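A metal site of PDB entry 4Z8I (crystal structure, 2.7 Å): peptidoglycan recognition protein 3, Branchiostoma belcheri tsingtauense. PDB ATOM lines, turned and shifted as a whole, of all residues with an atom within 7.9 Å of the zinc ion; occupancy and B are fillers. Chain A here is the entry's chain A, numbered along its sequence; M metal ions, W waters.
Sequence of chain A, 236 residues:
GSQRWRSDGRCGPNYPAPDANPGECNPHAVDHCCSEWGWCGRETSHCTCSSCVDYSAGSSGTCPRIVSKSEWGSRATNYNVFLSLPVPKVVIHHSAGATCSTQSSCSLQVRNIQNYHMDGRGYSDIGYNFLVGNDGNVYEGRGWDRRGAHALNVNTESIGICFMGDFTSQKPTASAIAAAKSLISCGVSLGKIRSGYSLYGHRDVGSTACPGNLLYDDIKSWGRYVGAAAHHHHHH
The backbone NH (N) of His 93 sits at hydrogen-bond distance from the backbone carbonyl oxygen (O) of Ile 161, 2.7 Å away. The backbone carbonyl oxygen (O) of Ile 92 lies within hydrogen-bond range of the backbone NH (N) of His 202, 3.1 Å away. O of Cys 210 is in hydrogen-bond range of N of Arg 203, 2.8 Å away. The backbone carbonyl oxygen of His 150 is in hydrogen-bond range of a ring nitrogen (NE2) of His 202 (3.4 Å). The backbone NH of His 94 sits close to the side-chain sulfur of Cys 210 (3.1 Å). A ring nitrogen (NE2) of His 93 lies within hydrogen-bond range of a ring nitrogen (ND1) of His 150 (2.9 Å). ND1 of His 202 lies close to OG1 of Thr 208, 3.3 Å away.
Within 4 Å of the zinc ion: His 93, His 202 and Cys 210. Along chain A the residues within 4 Å of the zinc ion span positions 93 to 210.
The zinc ion is bound by water W1 (1.9 Å), a ring nitrogen (ND1) of His 202 (2.0 Å), a ring nitrogen (ND1) of His 93 (2.0 Å) and the side-chain sulfur of Cys 210 (2.3 Å). The zinc ion has four donor atoms within binding distance.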
ATOM      1  N   VAL A  91      17.193  20.778  19.220  1.00  0.00           N
ATOM      2  CA  VAL A  91      15.856  20.366  18.786  1.00  0.00           C
ATOM      3  C   VAL A  91      15.721  18.854  18.869  1.00  0.00           C
ATOM      4  O   VAL A  91      16.583  18.121  18.383  1.00  0.00           O
ATOM      5  CB  VAL A  91      15.573  20.853  17.348  1.00  0.00           C
ATOM      6  CG1 VAL A  91      14.148  20.518  16.951  1.00  0.00           C
ATOM      7  CG2 VAL A  91      15.801  22.345  17.235  1.00  0.00           C
ATOM      8  N   ILE A  92      14.635  18.390  19.486  1.00  0.00           N
ATOM      9  CA  ILE A  92      14.411  16.964  19.677  1.00  0.00           C
ATOM     10  C   ILE A  92      13.410  16.421  18.662  1.00  0.00           C
ATOM     11  O   ILE A  92      12.337  17.000  18.453  1.00  0.00           O
ATOM     12  CB  ILE A  92      13.928  16.661  21.099  1.00  0.00           C
ATOM     13  CG1 ILE A  92      14.957  17.160  22.126  1.00  0.00           C
ATOM     14  CG2 ILE A  92      13.665  15.172  21.279  1.00  0.00           C
ATOM     15  CD1 ILE A  92      16.297  16.461  22.027  1.00  0.00           C
ATOM     16  N   HIS A  93      13.764  15.299  18.028  1.00  0.00           N
ATOM     17  CA  HIS A  93      12.932  14.703  16.991  1.00  0.00           C
ATOM     18  C   HIS A  93      12.560  13.276  17.344  1.00  0.00           C
ATOM     19  O   HIS A  93      13.223  12.643  18.158  1.00  0.00           O
ATOM     20  CB  HIS A  93      13.670  14.717  15.655  1.00  0.00           C
ATOM     21  CG  HIS A  93      13.848  16.076  15.066  1.00  0.00           C
ATOM     22  ND1 HIS A  93      12.933  16.636  14.200  1.00  0.00           N
ATOM     23  CD2 HIS A  93      14.832  16.986  15.216  1.00  0.00           C
ATOM     24  CE1 HIS A  93      13.348  17.840  13.840  1.00  0.00           C
ATOM     25  NE2 HIS A  93      14.502  18.076  14.450  1.00  0.00           N
ATOM     26  N   HIS A  94      11.495  12.765  16.727  1.00  0.00           N
ATOM     27  CA  HIS A  94      11.253  11.327  16.729  1.00  0.00           C
ATOM     28  C   HIS A  94      11.251  10.797  15.296  1.00  0.00           C
ATOM     29  O   HIS A  94      10.980  11.545  14.359  1.00  0.00           O
ATOM     30  CB  HIS A  94       9.983  10.937  17.511  1.00  0.00           C
ATOM     31  CG  HIS A  94       8.696  11.132  16.764  1.00  0.00           C
ATOM     32  ND1 HIS A  94       7.571  10.386  17.027  1.00  0.00           N
ATOM     33  CD2 HIS A  94       8.355  12.008  15.784  1.00  0.00           C
ATOM     34  CE1 HIS A  94       6.592  10.778  16.231  1.00  0.00           C
ATOM     35  NE2 HIS A  94       7.041  11.757  15.474  1.00  0.00           N
ATOM     36  N   SER A  95      11.566   9.523  15.133  1.00  0.00           N
ATOM     37  CA  SER A  95      11.648   8.923  13.805  1.00  0.00           C
ATOM     38  C   SER A  95      10.261   8.784  13.186  1.00  0.00           C
ATOM     39  O   SER A  95      10.120   8.727  11.963  1.00  0.00           O
ATOM     40  CB  SER A  95      12.314   7.555  13.883  1.00  0.00           C
ATOM     41  OG  SER A  95      12.201   6.851  12.661  1.00  0.00           O
ATOM     42  N   ALA A  96       9.236   8.745  14.041  1.00  0.00           N
ATOM     43  CA  ALA A  96       7.883   8.372  13.639  1.00  0.00           C
ATOM     44  C   ALA A  96       7.931   7.071  12.845  1.00  0.00           C
ATOM     45  O   ALA A  96       7.223   6.913  11.848  1.00  0.00           O
ATOM     46  CB  ALA A  96       7.230   9.481  12.824  1.00  0.00           C
ATOM     47  N   TYR A 128      19.544  14.394  10.434  1.00  0.00           N
ATOM     48  CA  TYR A 128      19.803  14.726  11.831  1.00  0.00           C
ATOM     49  C   TYR A 128      21.292  14.709  12.138  1.00  0.00           C
ATOM     50  O   TYR A 128      22.076  14.033  11.470  1.00  0.00           O
ATOM     51  CB  TYR A 128      19.058  13.747  12.736  1.00  0.00           C
ATOM     52  CG  TYR A 128      17.643  13.435  12.295  1.00  0.00           C
ATOM     53  CD1 TYR A 128      16.615  14.331  12.523  1.00  0.00           C
ATOM     54  CD2 TYR A 128      17.350  12.240  11.643  1.00  0.00           C
ATOM     55  CE1 TYR A 128      15.324  14.058  12.124  1.00  0.00           C
ATOM     56  CE2 TYR A 128      16.063  11.963  11.236  1.00  0.00           C
ATOM     57  CZ  TYR A 128      15.050  12.872  11.477  1.00  0.00           C
ATOM     58  OH  TYR A 128      13.775  12.582  11.070  1.00  0.00           O
ATOM     59  N   HIS A 150      16.844  19.153   9.591  1.00  0.00           N
ATOM     60  CA  HIS A 150      15.818  18.555  10.434  1.00  0.00           C
ATOM     61  C   HIS A 150      14.716  19.537  10.827  1.00  0.00           C
ATOM     62  O   HIS A 150      13.601  19.131  11.161  1.00  0.00           O
ATOM     63  CB  HIS A 150      16.458  17.968  11.697  1.00  0.00           C
ATOM     64  CG  HIS A 150      17.220  18.970  12.517  1.00  0.00           C
ATOM     65  ND1 HIS A 150      16.619  19.766  13.463  1.00  0.00           N
ATOM     66  CD2 HIS A 150      18.528  19.307  12.517  1.00  0.00           C
ATOM     67  CE1 HIS A 150      17.525  20.550  14.026  1.00  0.00           C
ATOM     68  NE2 HIS A 150      18.692  20.292  13.465  1.00  0.00           N
ATOM     69  N   ALA A 151      15.026  20.834  10.785  1.00  0.00           N
ATOM     70  CA  ALA A 151      14.049  21.869  11.126  1.00  0.00           C
ATOM     71  C   ALA A 151      14.413  23.190  10.453  1.00  0.00           C
ATOM     72  O   ALA A 151      15.331  23.881  10.885  1.00  0.00           O
ATOM     73  CB  ALA A 151      13.958  22.038  12.631  1.00  0.00           C
ATOM     74  N   ILE A 161      18.665  16.120  17.283  1.00  0.00           N
ATOM     75  CA  ILE A 161      18.732  14.772  17.829  1.00  0.00           C
ATOM     76  C   ILE A 161      17.418  14.042  17.589  1.00  0.00           C
ATOM     77  O   ILE A 161      16.353  14.528  17.980  1.00  0.00           O
ATOM     78  CB  ILE A 161      19.002  14.772  19.334  1.00  0.00           C
ATOM     79  CG1 ILE A 161      20.311  15.493  19.651  1.00  0.00           C
ATOM     80  CG2 ILE A 161      19.046  13.344  19.863  1.00  0.00           C
ATOM     81  CD1 ILE A 161      20.614  15.597  21.130  1.00  0.00           C
ATOM     82  N   CYS A 162      17.477  12.883  16.947  1.00  0.00           N
ATOM     83  CA  CYS A 162      16.267  12.134  16.634  1.00  0.00           C
ATOM     84  C   CYS A 162      16.233  10.787  17.340  1.00  0.00           C
ATOM     85  O   CYS A 162      17.108   9.950  17.127  1.00  0.00           O
ATOM     86  CB  CYS A 162      16.140  11.937  15.121  1.00  0.00           C
ATOM     87  SG  CYS A 162      14.706  10.958  14.642  1.00  0.00           S
ATOM     88  N   GLY A 201      11.323  20.987  21.282  1.00  0.00           N
ATOM     89  CA  GLY A 201      10.798  19.871  20.532  1.00  0.00           C
ATOM     90  C   GLY A 201      10.615  20.370  19.114  1.00  0.00           C
ATOM     91  O   GLY A 201      10.571  21.577  18.891  1.00  0.00           O
ATOM     92  N   HIS A 202      10.525  19.464  18.149  1.00  0.00           N
ATOM     93  CA  HIS A 202      10.367  19.869  16.756  1.00  0.00           C
ATOM     94  C   HIS A 202       9.091  20.692  16.561  1.00  0.00           C
ATOM     95  O   HIS A 202       9.082  21.671  15.806  1.00  0.00           O
ATOM     96  CB  HIS A 202      10.356  18.643  15.829  1.00  0.00           C
ATOM     97  CG  HIS A 202      10.406  18.983  14.378  1.00  0.00           C
ATOM     98  ND1 HIS A 202      10.205  18.033  13.392  1.00  0.00           N
ATOM     99  CD2 HIS A 202      10.639  20.151  13.733  1.00  0.00           C
ATOM    100  CE1 HIS A 202      10.309  18.610  12.203  1.00  0.00           C
ATOM    101  NE2 HIS A 202      10.567  19.892  12.380  1.00  0.00           N
ATOM    102  N   ARG A 203       8.030  20.304  17.261  1.00  0.00           N
ATOM    103  CA  ARG A 203       6.742  20.997  17.142  1.00  0.00           C
ATOM    104  C   ARG A 203       6.812  22.423  17.668  1.00  0.00           C
ATOM    105  O   ARG A 203       5.977  23.264  17.326  1.00  0.00           O
ATOM    106  CB  ARG A 203       5.653  20.228  17.896  1.00  0.00           C
ATOM    107  CG  ARG A 203       5.900  20.115  19.388  1.00  0.00           C
ATOM    108  CD  ARG A 203       4.727  19.456  20.102  1.00  0.00           C
ATOM    109  NE  ARG A 203       4.480  18.100  19.635  1.00  0.00           N
ATOM    110  CZ  ARG A 203       3.516  17.309  20.091  1.00  0.00           C
ATOM    111  NH1 ARG A 203       2.699  17.751  21.043  1.00  0.00           N
ATOM    112  NH2 ARG A 203       3.362  16.086  19.612  1.00  0.00           N
ATOM    113  N   VAL A 205       9.120  24.516  16.998  1.00  0.00           N
ATOM    114  CA  VAL A 205       9.803  25.355  16.025  1.00  0.00           C
ATOM    115  C   VAL A 205       9.258  25.158  14.609  1.00  0.00           C
ATOM    116  O   VAL A 205       9.604  25.898  13.691  1.00  0.00           O
ATOM    117  CB  VAL A 205      11.316  25.076  16.049  1.00  0.00           C
ATOM    118  CG1 VAL A 205      11.615  23.773  15.333  1.00  0.00           C
ATOM    119  CG2 VAL A 205      12.107  26.225  15.449  1.00  0.00           C
ATOM    120  N   THR A 208       4.708  20.118  13.046  1.00  0.00           N
ATOM    121  CA  THR A 208       4.634  18.657  13.046  1.00  0.00           C
ATOM    122  C   THR A 208       4.093  18.156  14.370  1.00  0.00           C
ATOM    123  O   THR A 208       3.881  18.937  15.298  1.00  0.00           O
ATOM    124  CB  THR A 208       6.018  18.023  12.810  1.00  0.00           C
ATOM    125  OG1 THR A 208       7.002  18.637  13.652  1.00  0.00           O
ATOM    126  CG2 THR A 208       6.448  18.172  11.369  1.00  0.00           C
ATOM    127  N   ALA A 209       3.849  16.855  14.459  1.00  0.00           N
ATOM    128  CA  ALA A 209       3.525  16.235  15.734  1.00  0.00           C
ATOM    129  C   ALA A 209       4.813  15.742  16.381  1.00  0.00           C
ATOM    130  O   ALA A 209       4.806  15.239  17.505  1.00  0.00           O
ATOM    131  CB  ALA A 209       2.551  15.090  15.530  1.00  0.00           C
ATOM    132  N   CYS A 210       5.918  15.876  15.652  1.00  0.00           N
ATOM    133  CA  CYS A 210       7.237  15.526  16.163  1.00  0.00           C
ATOM    134  C   CYS A 210       7.543  16.375  17.393  1.00  0.00           C
ATOM    135  O   CYS A 210       7.257  17.570  17.390  1.00  0.00           O
ATOM    136  CB  CYS A 210       8.287  15.786  15.065  1.00  0.00           C
ATOM    137  SG  CYS A 210       9.898  15.026  15.323  1.00  0.00           S
ATOM    138  N   PRO A 211       8.140  15.774  18.430  1.00  0.00           N
ATOM    139  CA  PRO A 211       8.666  14.406  18.499  1.00  0.00           C
ATOM    140  C   PRO A 211       7.681  13.417  19.101  1.00  0.00           C
ATOM    141  O   PRO A 211       8.121  12.496  19.794  1.00  0.00           O
ATOM    142  CB  PRO A 211       9.850  14.570  19.437  1.00  0.00           C
ATOM    143  CG  PRO A 211       9.373  15.589  20.413  1.00  0.00           C
ATOM    144  CD  PRO A 211       8.477  16.533  19.649  1.00  0.00           C
ATOM    145  N   GLY A 212       6.385  13.596  18.868  1.00  0.00           N
ATOM    146  CA  GLY A 212       5.381  12.736  19.477  1.00  0.00           C
ATOM    147  C   GLY A 212       4.972  13.236  20.841  1.00  0.00           C
ATOM    148  O   GLY A 212       5.788  13.802  21.575  1.00  0.00           O
HETATM  149 ZN    ZN M   1      10.994  16.291  13.808  1.00  0.00          ZN
HETATM  150  O   HOH W   1      11.417  15.579  12.043  1.00  0.00           O
